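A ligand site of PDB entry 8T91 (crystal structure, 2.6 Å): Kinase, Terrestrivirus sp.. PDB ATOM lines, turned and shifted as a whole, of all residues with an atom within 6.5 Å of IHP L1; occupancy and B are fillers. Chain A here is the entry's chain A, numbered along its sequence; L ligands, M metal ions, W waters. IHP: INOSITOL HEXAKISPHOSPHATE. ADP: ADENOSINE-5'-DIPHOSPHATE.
An oxygen (O46) of IHP L1 is in salt-bridge range of the guanidinium group (NE) of Arg 116 (2.8 Å).
An oxygen (O25) of IHP L1 is in hydrogen-bond range of the backbone NH (N) of Arg 118 (3.4 Å).
The guanidinium group of Arg 118 is in salt-bridge range of an oxygen (O34) of IHP L1, at 2.8 Å.
The side-chain amino group (NZ) of Lys 60 lies within salt-bridge range of an oxygen (O23) of IHP L1, at 2.8 Å.
An oxygen (O36) of IHP L1 is in hydrogen-bond range of the backbone NH of Lys 117 (3.1 Å).
NZ of Lys 117 lies within salt-bridge range of O24 of IHP L1, 2.9 Å away.
NZ of Lys 112 lies within salt-bridge range of O46 of IHP L1 (3.0 Å).
NE of Arg 42 is in salt-bridge range of O33 of IHP L1, 3.5 Å away.
The guanidinium group (NH1) of Arg 218 lies within salt-bridge range of an oxygen (O36) of IHP L1 (3.0 Å).
The backbone NH (N) of Arg 42 sits at hydrogen-bond distance from an oxygen (O2B) of ADP L2 (3.1 Å).
The backbone NH (N) of Ala 40 is in hydrogen-bond range of an oxygen (O3') of ADP L2 (3.1 Å).
The backbone NH of Ser 43 lies close to an oxygen (O2B) of ADP L2, at 3.0 Å.
The side-chain hydroxyl (OG) of Ser 43 sits at hydrogen-bond distance from an oxygen (O2B) of ADP L2.
An oxygen (O3') of ADP L2 sits at hydrogen-bond distance from the side-chain carboxylate of Asp 110, 2.7 Å away.
The backbone NH (N) of Lys 112 is in hydrogen-bond range of the backbone carbonyl oxygen (O) of Ser 127.
The backbone carbonyl oxygen (O) of Ala 115 lies within hydrogen-bond range of the guanidinium group (NH2) of Arg 218, at 2.8 Å.
Gly 41 touches IHP L1 (CA to O31, 3.5 Å).
CG of Lys 119 touches O25 of IHP L1, 3.5 Å away.
Within 4 Å of IHP L1: Gly 41, Arg 42, Lys 60, Lys 112, Arg 116, Lys 117, Arg 118, Lys 119 and Arg 218.
Along chain A the residues within 4 Å of IHP L1 span positions 41 to 218.
The nearest printed residue that does not touch IHP L1 is Arg 129 (4.01 Å).
Water W7 lies within hydrogen-bond range of the side-chain hydroxyl (OG) of Ser 217 (2.8 Å), the side-chain carboxylate (OD1) of Asp 215 (3.1 Å) and an oxygen (O22) of IHP L1 (3.2 Å).
Water W2 bridges NH1 of Arg 42 (2.8 Å) and O14 of IHP L1 (3.4 Å).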
ATOM      1  N   ALA A  40      20.295  -9.768 -13.858  1.00  0.00           N
ATOM      2  CA  ALA A  40      19.848 -10.235 -12.519  1.00  0.00           C
ATOM      3  C   ALA A  40      20.916 -11.138 -11.874  1.00  0.00           C
ATOM      4  O   ALA A  40      22.082 -11.116 -12.328  1.00  0.00           O
ATOM      5  CB  ALA A  40      18.526 -10.946 -12.648  1.00  0.00           C
ATOM      6  N   GLY A  41      20.516 -11.891 -10.851  1.00  0.00           N
ATOM      7  CA  GLY A  41      21.407 -12.803 -10.097  1.00  0.00           C
ATOM      8  C   GLY A  41      22.294 -12.023  -9.160  1.00  0.00           C
ATOM      9  O   GLY A  41      22.064 -10.806  -8.997  1.00  0.00           O
ATOM     10  N   ARG A  42      23.297 -12.685  -8.575  1.00  0.00           N
ATOM     11  CA  ARG A  42      24.243 -12.092  -7.597  1.00  0.00           C
ATOM     12  C   ARG A  42      25.661 -12.651  -7.810  1.00  0.00           C
ATOM     13  O   ARG A  42      26.527 -12.370  -6.954  1.00  0.00           O
ATOM     14  CB  ARG A  42      23.666 -12.303  -6.187  1.00  0.00           C
ATOM     15  CG  ARG A  42      22.645 -11.247  -5.796  1.00  0.00           C
ATOM     16  CD  ARG A  42      21.293 -11.795  -5.357  1.00  0.00           C
ATOM     17  NE  ARG A  42      20.846 -11.171  -4.118  1.00  0.00           N
ATOM     18  CZ  ARG A  42      19.584 -11.138  -3.656  1.00  0.00           C
ATOM     19  NH1 ARG A  42      19.317 -10.537  -2.514  1.00  0.00           N
ATOM     20  NH2 ARG A  42      18.593 -11.687  -4.345  1.00  0.00           N
ATOM     21  N   SER A  43      25.915 -13.344  -8.924  1.00  0.00           N
ATOM     22  CA  SER A  43      27.185 -14.072  -9.228  1.00  0.00           C
ATOM     23  C   SER A  43      28.187 -13.147  -9.918  1.00  0.00           C
ATOM     24  O   SER A  43      27.774 -12.292 -10.731  1.00  0.00           O
ATOM     25  CB  SER A  43      26.936 -15.301 -10.070  1.00  0.00           C
ATOM     26  OG  SER A  43      26.294 -16.329  -9.330  1.00  0.00           O
ATOM     27  N   LYS A  60      29.232 -21.004  -4.011  1.00  0.00           N
ATOM     28  CA  LYS A  60      28.910 -21.781  -2.777  1.00  0.00           C
ATOM     29  C   LYS A  60      29.392 -23.224  -2.947  1.00  0.00           C
ATOM     30  O   LYS A  60      29.973 -23.763  -1.993  1.00  0.00           O
ATOM     31  CB  LYS A  60      27.423 -21.623  -2.471  1.00  0.00           C
ATOM     32  CG  LYS A  60      26.926 -20.192  -2.701  1.00  0.00           C
ATOM     33  CD  LYS A  60      25.660 -19.772  -2.012  1.00  0.00           C
ATOM     34  CE  LYS A  60      25.471 -18.280  -2.120  1.00  0.00           C
ATOM     35  NZ  LYS A  60      24.080 -17.856  -1.884  1.00  0.00           N
ATOM     36  N   ASP A 110      15.413 -11.622 -17.687  1.00  0.00           N
ATOM     37  CA  ASP A 110      15.621 -12.797 -16.811  1.00  0.00           C
ATOM     38  C   ASP A 110      14.289 -13.069 -16.128  1.00  0.00           C
ATOM     39  O   ASP A 110      13.805 -12.188 -15.409  1.00  0.00           O
ATOM     40  CB  ASP A 110      16.768 -12.566 -15.807  1.00  0.00           C
ATOM     41  CG  ASP A 110      17.085 -13.757 -14.919  1.00  0.00           C
ATOM     42  OD1 ASP A 110      16.156 -14.503 -14.564  1.00  0.00           O
ATOM     43  OD2 ASP A 110      18.268 -13.901 -14.553  1.00  0.00           O
ATOM     44  N   LYS A 112      12.787 -16.009 -13.578  1.00  0.00           N
ATOM     45  CA  LYS A 112      12.968 -17.214 -12.712  1.00  0.00           C
ATOM     46  C   LYS A 112      11.707 -18.069 -12.858  1.00  0.00           C
ATOM     47  O   LYS A 112      10.648 -17.605 -12.466  1.00  0.00           O
ATOM     48  CB  LYS A 112      13.238 -16.791 -11.260  1.00  0.00           C
ATOM     49  CG  LYS A 112      13.562 -17.927 -10.297  1.00  0.00           C
ATOM     50  CD  LYS A 112      15.021 -18.040  -9.925  1.00  0.00           C
ATOM     51  CE  LYS A 112      15.489 -16.980  -8.953  1.00  0.00           C
ATOM     52  NZ  LYS A 112      16.443 -17.532  -7.951  1.00  0.00           N
ATOM     53  N   ALA A 115      11.611 -22.960  -8.704  1.00  0.00           N
ATOM     54  CA  ALA A 115      11.225 -22.564  -7.327  1.00  0.00           C
ATOM     55  C   ALA A 115      12.286 -21.593  -6.808  1.00  0.00           C
ATOM     56  O   ALA A 115      13.470 -21.784  -7.119  1.00  0.00           O
ATOM     57  CB  ALA A 115      11.096 -23.783  -6.433  1.00  0.00           C
ATOM     58  N   ARG A 116      11.834 -20.571  -6.075  1.00  0.00           N
ATOM     59  CA  ARG A 116      12.702 -19.658  -5.286  1.00  0.00           C
ATOM     60  C   ARG A 116      13.025 -20.363  -3.977  1.00  0.00           C
ATOM     61  O   ARG A 116      12.384 -21.387  -3.706  1.00  0.00           O
ATOM     62  CB  ARG A 116      11.976 -18.331  -5.081  1.00  0.00           C
ATOM     63  CG  ARG A 116      11.461 -17.727  -6.390  1.00  0.00           C
ATOM     64  CD  ARG A 116      10.907 -16.340  -6.193  1.00  0.00           C
ATOM     65  NE  ARG A 116      11.973 -15.373  -5.975  1.00  0.00           N
ATOM     66  CZ  ARG A 116      11.790 -14.124  -5.560  1.00  0.00           C
ATOM     67  NH1 ARG A 116      10.575 -13.666  -5.303  1.00  0.00           N
ATOM     68  NH2 ARG A 116      12.830 -13.327  -5.397  1.00  0.00           N
ATOM     69  N   LYS A 117      14.021 -19.910  -3.212  1.00  0.00           N
ATOM     70  CA  LYS A 117      14.439 -20.616  -1.983  1.00  0.00           C
ATOM     71  C   LYS A 117      13.319 -20.515  -0.937  1.00  0.00           C
ATOM     72  O   LYS A 117      12.867 -21.559  -0.480  1.00  0.00           O
ATOM     73  CB  LYS A 117      15.756 -20.073  -1.436  1.00  0.00           C
ATOM     74  CG  LYS A 117      16.973 -20.422  -2.257  1.00  0.00           C
ATOM     75  CD  LYS A 117      18.162 -19.541  -1.984  1.00  0.00           C
ATOM     76  CE  LYS A 117      18.868 -19.895  -0.692  1.00  0.00           C
ATOM     77  NZ  LYS A 117      20.271 -19.422  -0.719  1.00  0.00           N
ATOM     78  N   ARG A 118      12.873 -19.311  -0.596  1.00  0.00           N
ATOM     79  CA  ARG A 118      11.822 -19.099   0.446  1.00  0.00           C
ATOM     80  C   ARG A 118      10.591 -18.492  -0.213  1.00  0.00           C
ATOM     81  O   ARG A 118       9.547 -19.166  -0.279  1.00  0.00           O
ATOM     82  CB  ARG A 118      12.301 -18.161   1.564  1.00  0.00           C
ATOM     83  CG  ARG A 118      13.041 -18.867   2.698  1.00  0.00           C
ATOM     84  CD  ARG A 118      14.523 -18.526   2.746  1.00  0.00           C
ATOM     85  NE  ARG A 118      15.328 -19.715   2.991  1.00  0.00           N
ATOM     86  CZ  ARG A 118      16.655 -19.747   3.047  1.00  0.00           C
ATOM     87  NH1 ARG A 118      17.361 -18.635   2.902  1.00  0.00           N
ATOM     88  NH2 ARG A 118      17.271 -20.894   3.261  1.00  0.00           N
ATOM     89  N   LYS A 119      10.750 -17.257  -0.691  1.00  0.00           N
ATOM     90  CA  LYS A 119       9.674 -16.412  -1.292  1.00  0.00           C
ATOM     91  C   LYS A 119       8.841 -17.255  -2.252  1.00  0.00           C
ATOM     92  O   LYS A 119       9.404 -18.124  -2.929  1.00  0.00           O
ATOM     93  CB  LYS A 119      10.298 -15.218  -2.016  1.00  0.00           C
ATOM     94  CG  LYS A 119      11.392 -14.490  -1.247  1.00  0.00           C
ATOM     95  CD  LYS A 119      11.672 -13.103  -1.752  1.00  0.00           C
ATOM     96  CE  LYS A 119      12.430 -12.260  -0.742  1.00  0.00           C
ATOM     97  NZ  LYS A 119      12.754 -10.929  -1.290  1.00  0.00           N
ATOM     98  N   SER A 127       8.751 -15.303 -11.613  1.00  0.00           N
ATOM     99  CA  SER A 127       9.227 -13.985 -11.139  1.00  0.00           C
ATOM    100  C   SER A 127      10.164 -13.393 -12.200  1.00  0.00           C
ATOM    101  O   SER A 127      11.255 -13.943 -12.390  1.00  0.00           O
ATOM    102  CB  SER A 127       9.940 -14.126  -9.819  1.00  0.00           C
ATOM    103  OG  SER A 127       9.172 -14.903  -8.918  1.00  0.00           O
ATOM    104  N   ARG A 129      13.013 -11.259 -12.947  1.00  0.00           N
ATOM    105  CA  ARG A 129      14.092 -10.781 -12.049  1.00  0.00           C
ATOM    106  C   ARG A 129      14.668  -9.479 -12.589  1.00  0.00           C
ATOM    107  O   ARG A 129      15.246  -8.753 -11.781  1.00  0.00           O
ATOM    108  CB  ARG A 129      15.218 -11.809 -11.930  1.00  0.00           C
ATOM    109  CG  ARG A 129      14.755 -13.201 -11.541  1.00  0.00           C
ATOM    110  CD  ARG A 129      13.846 -13.232 -10.330  1.00  0.00           C
ATOM    111  NE  ARG A 129      14.348 -12.584  -9.111  1.00  0.00           N
ATOM    112  CZ  ARG A 129      13.663 -11.671  -8.392  1.00  0.00           C
ATOM    113  NH1 ARG A 129      14.207 -11.192  -7.290  1.00  0.00           N
ATOM    114  NH2 ARG A 129      12.458 -11.260  -8.759  1.00  0.00           N
ATOM    115  N   GLY A 195      15.382 -22.671  -9.066  1.00  0.00           N
ATOM    116  CA  GLY A 195      16.132 -21.417  -9.239  1.00  0.00           C
ATOM    117  C   GLY A 195      16.599 -21.172 -10.659  1.00  0.00           C
ATOM    118  O   GLY A 195      17.281 -20.149 -10.854  1.00  0.00           O
ATOM    119  N   SER A 197      16.466 -19.918 -14.579  1.00  0.00           N
ATOM    120  CA  SER A 197      15.831 -18.770 -15.248  1.00  0.00           C
ATOM    121  C   SER A 197      15.739 -19.047 -16.740  1.00  0.00           C
ATOM    122  O   SER A 197      16.516 -19.886 -17.243  1.00  0.00           O
ATOM    123  CB  SER A 197      16.581 -17.475 -14.993  1.00  0.00           C
ATOM    124  OG  SER A 197      16.281 -16.975 -13.708  1.00  0.00           O
ATOM    125  N   ASP A 215      21.341 -21.232 -15.146  1.00  0.00           N
ATOM    126  CA  ASP A 215      21.548 -21.248 -13.675  1.00  0.00           C
ATOM    127  C   ASP A 215      21.083 -22.580 -13.109  1.00  0.00           C
ATOM    128  O   ASP A 215      19.923 -22.678 -12.656  1.00  0.00           O
ATOM    129  CB  ASP A 215      20.868 -20.063 -12.982  1.00  0.00           C
ATOM    130  CG  ASP A 215      21.322 -19.823 -11.555  1.00  0.00           C
ATOM    131  OD1 ASP A 215      22.114 -20.649 -11.036  1.00  0.00           O
ATOM    132  OD2 ASP A 215      20.897 -18.803 -10.977  1.00  0.00           O
ATOM    133  N   SER A 217      22.650 -24.084 -10.558  1.00  0.00           N
ATOM    134  CA  SER A 217      23.402 -24.125  -9.274  1.00  0.00           C
ATOM    135  C   SER A 217      22.607 -24.888  -8.209  1.00  0.00           C
ATOM    136  O   SER A 217      23.262 -25.597  -7.445  1.00  0.00           O
ATOM    137  CB  SER A 217      23.731 -22.746  -8.808  1.00  0.00           C
ATOM    138  OG  SER A 217      22.540 -22.003  -8.581  1.00  0.00           O
ATOM    139  N   ARG A 218      21.284 -24.755  -8.176  1.00  0.00           N
ATOM    140  CA  ARG A 218      20.376 -25.381  -7.162  1.00  0.00           C
ATOM    141  C   ARG A 218      19.521 -26.506  -7.778  1.00  0.00           C
ATOM    142  O   ARG A 218      18.532 -26.918  -7.130  1.00  0.00           O
ATOM    143  CB  ARG A 218      19.447 -24.327  -6.542  1.00  0.00           C
ATOM    144  CG  ARG A 218      20.140 -23.299  -5.654  1.00  0.00           C
ATOM    145  CD  ARG A 218      19.253 -22.101  -5.342  1.00  0.00           C
ATOM    146  NE  ARG A 218      17.852 -22.488  -5.157  1.00  0.00           N
ATOM    147  CZ  ARG A 218      16.778 -21.749  -5.503  1.00  0.00           C
ATOM    148  NH1 ARG A 218      16.900 -20.544  -6.043  1.00  0.00           N
ATOM    149  NH2 ARG A 218      15.572 -22.236  -5.285  1.00  0.00           N
HETATM  150  C1  IHP L   1      18.759 -15.533  -4.943  1.00  0.00           C
HETATM  151  C2  IHP L   1      20.057 -16.102  -4.420  1.00  0.00           C
HETATM  152  C3  IHP L   1      20.279 -15.463  -2.998  1.00  0.00           C
HETATM  153  C4  IHP L   1      19.108 -15.821  -1.993  1.00  0.00           C
HETATM  154  C5  IHP L   1      17.739 -15.497  -2.606  1.00  0.00           C
HETATM  155  C6  IHP L   1      17.628 -16.022  -4.034  1.00  0.00           C
HETATM  156  O11 IHP L   1      18.604 -15.868  -6.372  1.00  0.00           O
HETATM  157  P1  IHP L   1      19.013 -14.770  -7.504  1.00  0.00           P
HETATM  158  O21 IHP L   1      17.781 -13.785  -7.419  1.00  0.00           O
HETATM  159  O31 IHP L   1      20.382 -14.132  -7.027  1.00  0.00           O
HETATM  160  O41 IHP L   1      19.089 -15.554  -8.744  1.00  0.00           O
HETATM  161  O12 IHP L   1      20.017 -17.553  -4.395  1.00  0.00           O
HETATM  162  P2  IHP L   1      21.338 -18.409  -4.726  1.00  0.00           P
HETATM  163  O22 IHP L   1      20.928 -18.863  -6.188  1.00  0.00           O
HETATM  164  O32 IHP L   1      21.437 -19.590  -3.666  1.00  0.00           O
HETATM  165  O42 IHP L   1      22.441 -17.417  -4.693  1.00  0.00           O
HETATM  166  O13 IHP L   1      21.580 -15.796  -2.451  1.00  0.00           O
HETATM  167  P3  IHP L   1      22.657 -14.619  -2.371  1.00  0.00           P
HETATM  168  O23 IHP L   1      23.822 -15.092  -1.420  1.00  0.00           O
HETATM  169  O33 IHP L   1      21.787 -13.476  -1.691  1.00  0.00           O
HETATM  170  O43 IHP L   1      22.971 -14.234  -3.781  1.00  0.00           O
HETATM  171  O14 IHP L   1      19.241 -15.132  -0.703  1.00  0.00           O
HETATM  172  P4  IHP L   1      19.430 -15.958   0.704  1.00  0.00           P
HETATM  173  O24 IHP L   1      20.728 -16.876   0.496  1.00  0.00           O
HETATM  174  O34 IHP L   1      18.204 -16.947   0.866  1.00  0.00           O
HETATM  175  O44 IHP L   1      19.751 -14.995   1.811  1.00  0.00           O
HETATM  176  O15 IHP L   1      16.723 -16.153  -1.794  1.00  0.00           O
HETATM  177  P5  IHP L   1      15.528 -15.449  -0.954  1.00  0.00           P
HETATM  178  O25 IHP L   1      14.335 -16.396  -1.407  1.00  0.00           O
HETATM  179  O35 IHP L   1      15.436 -13.953  -1.475  1.00  0.00           O
HETATM  180  O45 IHP L   1      15.876 -15.643   0.488  1.00  0.00           O
HETATM  181  O16 IHP L   1      16.430 -15.504  -4.508  1.00  0.00           O
HETATM  182  P6  IHP L   1      15.243 -16.471  -4.994  1.00  0.00           P
HETATM  183  O26 IHP L   1      14.234 -16.258  -3.835  1.00  0.00           O
HETATM  184  O36 IHP L   1      15.719 -17.977  -4.977  1.00  0.00           O
HETATM  185  O46 IHP L   1      14.681 -15.858  -6.261  1.00  0.00           O
HETATM  186  PB  ADP L   2      23.094 -16.344 -10.754  1.00  0.00           P
HETATM  187  O1B ADP L   2      21.623 -16.007 -10.666  1.00  0.00           O
HETATM  188  O2B ADP L   2      23.953 -15.281 -10.153  1.00  0.00           O
HETATM  189  O3B ADP L   2      23.414 -17.744 -10.216  1.00  0.00           O
HETATM  190  PA  ADP L   2      22.588 -16.638 -13.666  1.00  0.00           P
HETATM  191  O1A ADP L   2      21.113 -16.662 -13.389  1.00  0.00           O
HETATM  192  O2A ADP L   2      23.214 -17.833 -14.306  1.00  0.00           O
HETATM  193  O3A ADP L   2      23.434 -16.310 -12.333  1.00  0.00           O
HETATM  194  O5' ADP L   2      22.931 -15.341 -14.544  1.00  0.00           O
HETATM  195  C5' ADP L   2      22.544 -14.047 -14.048  1.00  0.00           C
HETATM  196  C4' ADP L   2      22.472 -13.086 -15.201  1.00  0.00           C
HETATM  197  O4' ADP L   2      23.612 -13.306 -16.072  1.00  0.00           O
HETATM  198  C3' ADP L   2      21.244 -13.224 -16.111  1.00  0.00           C
HETATM  199  O3' ADP L   2      20.222 -12.364 -15.639  1.00  0.00           O
HETATM  200  C2' ADP L   2      21.778 -12.798 -17.485  1.00  0.00           C
HETATM  201  O2' ADP L   2      21.668 -11.414 -17.714  1.00  0.00           O
HETATM  202  C1' ADP L   2      23.255 -13.199 -17.428  1.00  0.00           C
HETATM  203  N9  ADP L   2      23.616 -14.453 -18.075  1.00  0.00           N
HETATM  204  C8  ADP L   2      23.728 -15.693 -17.488  1.00  0.00           C
HETATM  205  N7  ADP L   2      24.131 -16.626 -18.310  1.00  0.00           N
HETATM  206  C5  ADP L   2      24.323 -15.972 -19.516  1.00  0.00           C
HETATM  207  C6  ADP L   2      24.761 -16.412 -20.778  1.00  0.00           C
HETATM  208  N6  ADP L   2      25.116 -17.666 -21.045  1.00  0.00           N
HETATM  209  N1  ADP L   2      24.866 -15.483 -21.753  1.00  0.00           N
HETATM  210  C2  ADP L   2      24.525 -14.217 -21.477  1.00  0.00           C
HETATM  211  N3  ADP L   2      24.086 -13.687 -20.336  1.00  0.00           N
HETATM  212  C4  ADP L   2      24.017 -14.629 -19.378  1.00  0.00           C
HETATM  213 MG    MG M   1      20.005 -16.802 -11.482  1.00  0.00          MG
HETATM  214  O   HOH W   1      24.483 -19.702  -6.077  1.00  0.00           O
HETATM  215  O   HOH W   2      18.077 -11.916  -0.420  1.00  0.00           O
HETATM  216  O   HOH W   3      20.722 -22.252  -2.858  1.00  0.00           O
HETATM  217  O   HOH W   4      25.942 -15.268  -0.124  1.00  0.00           O
HETATM  218  O   HOH W   5      17.684 -14.139 -10.209  1.00  0.00           O
HETATM  219  O   HOH W   6      19.360 -15.495   4.329  1.00  0.00           O
HETATM  220  O   HOH W   7      20.065 -20.770  -8.652  1.00  0.00           O
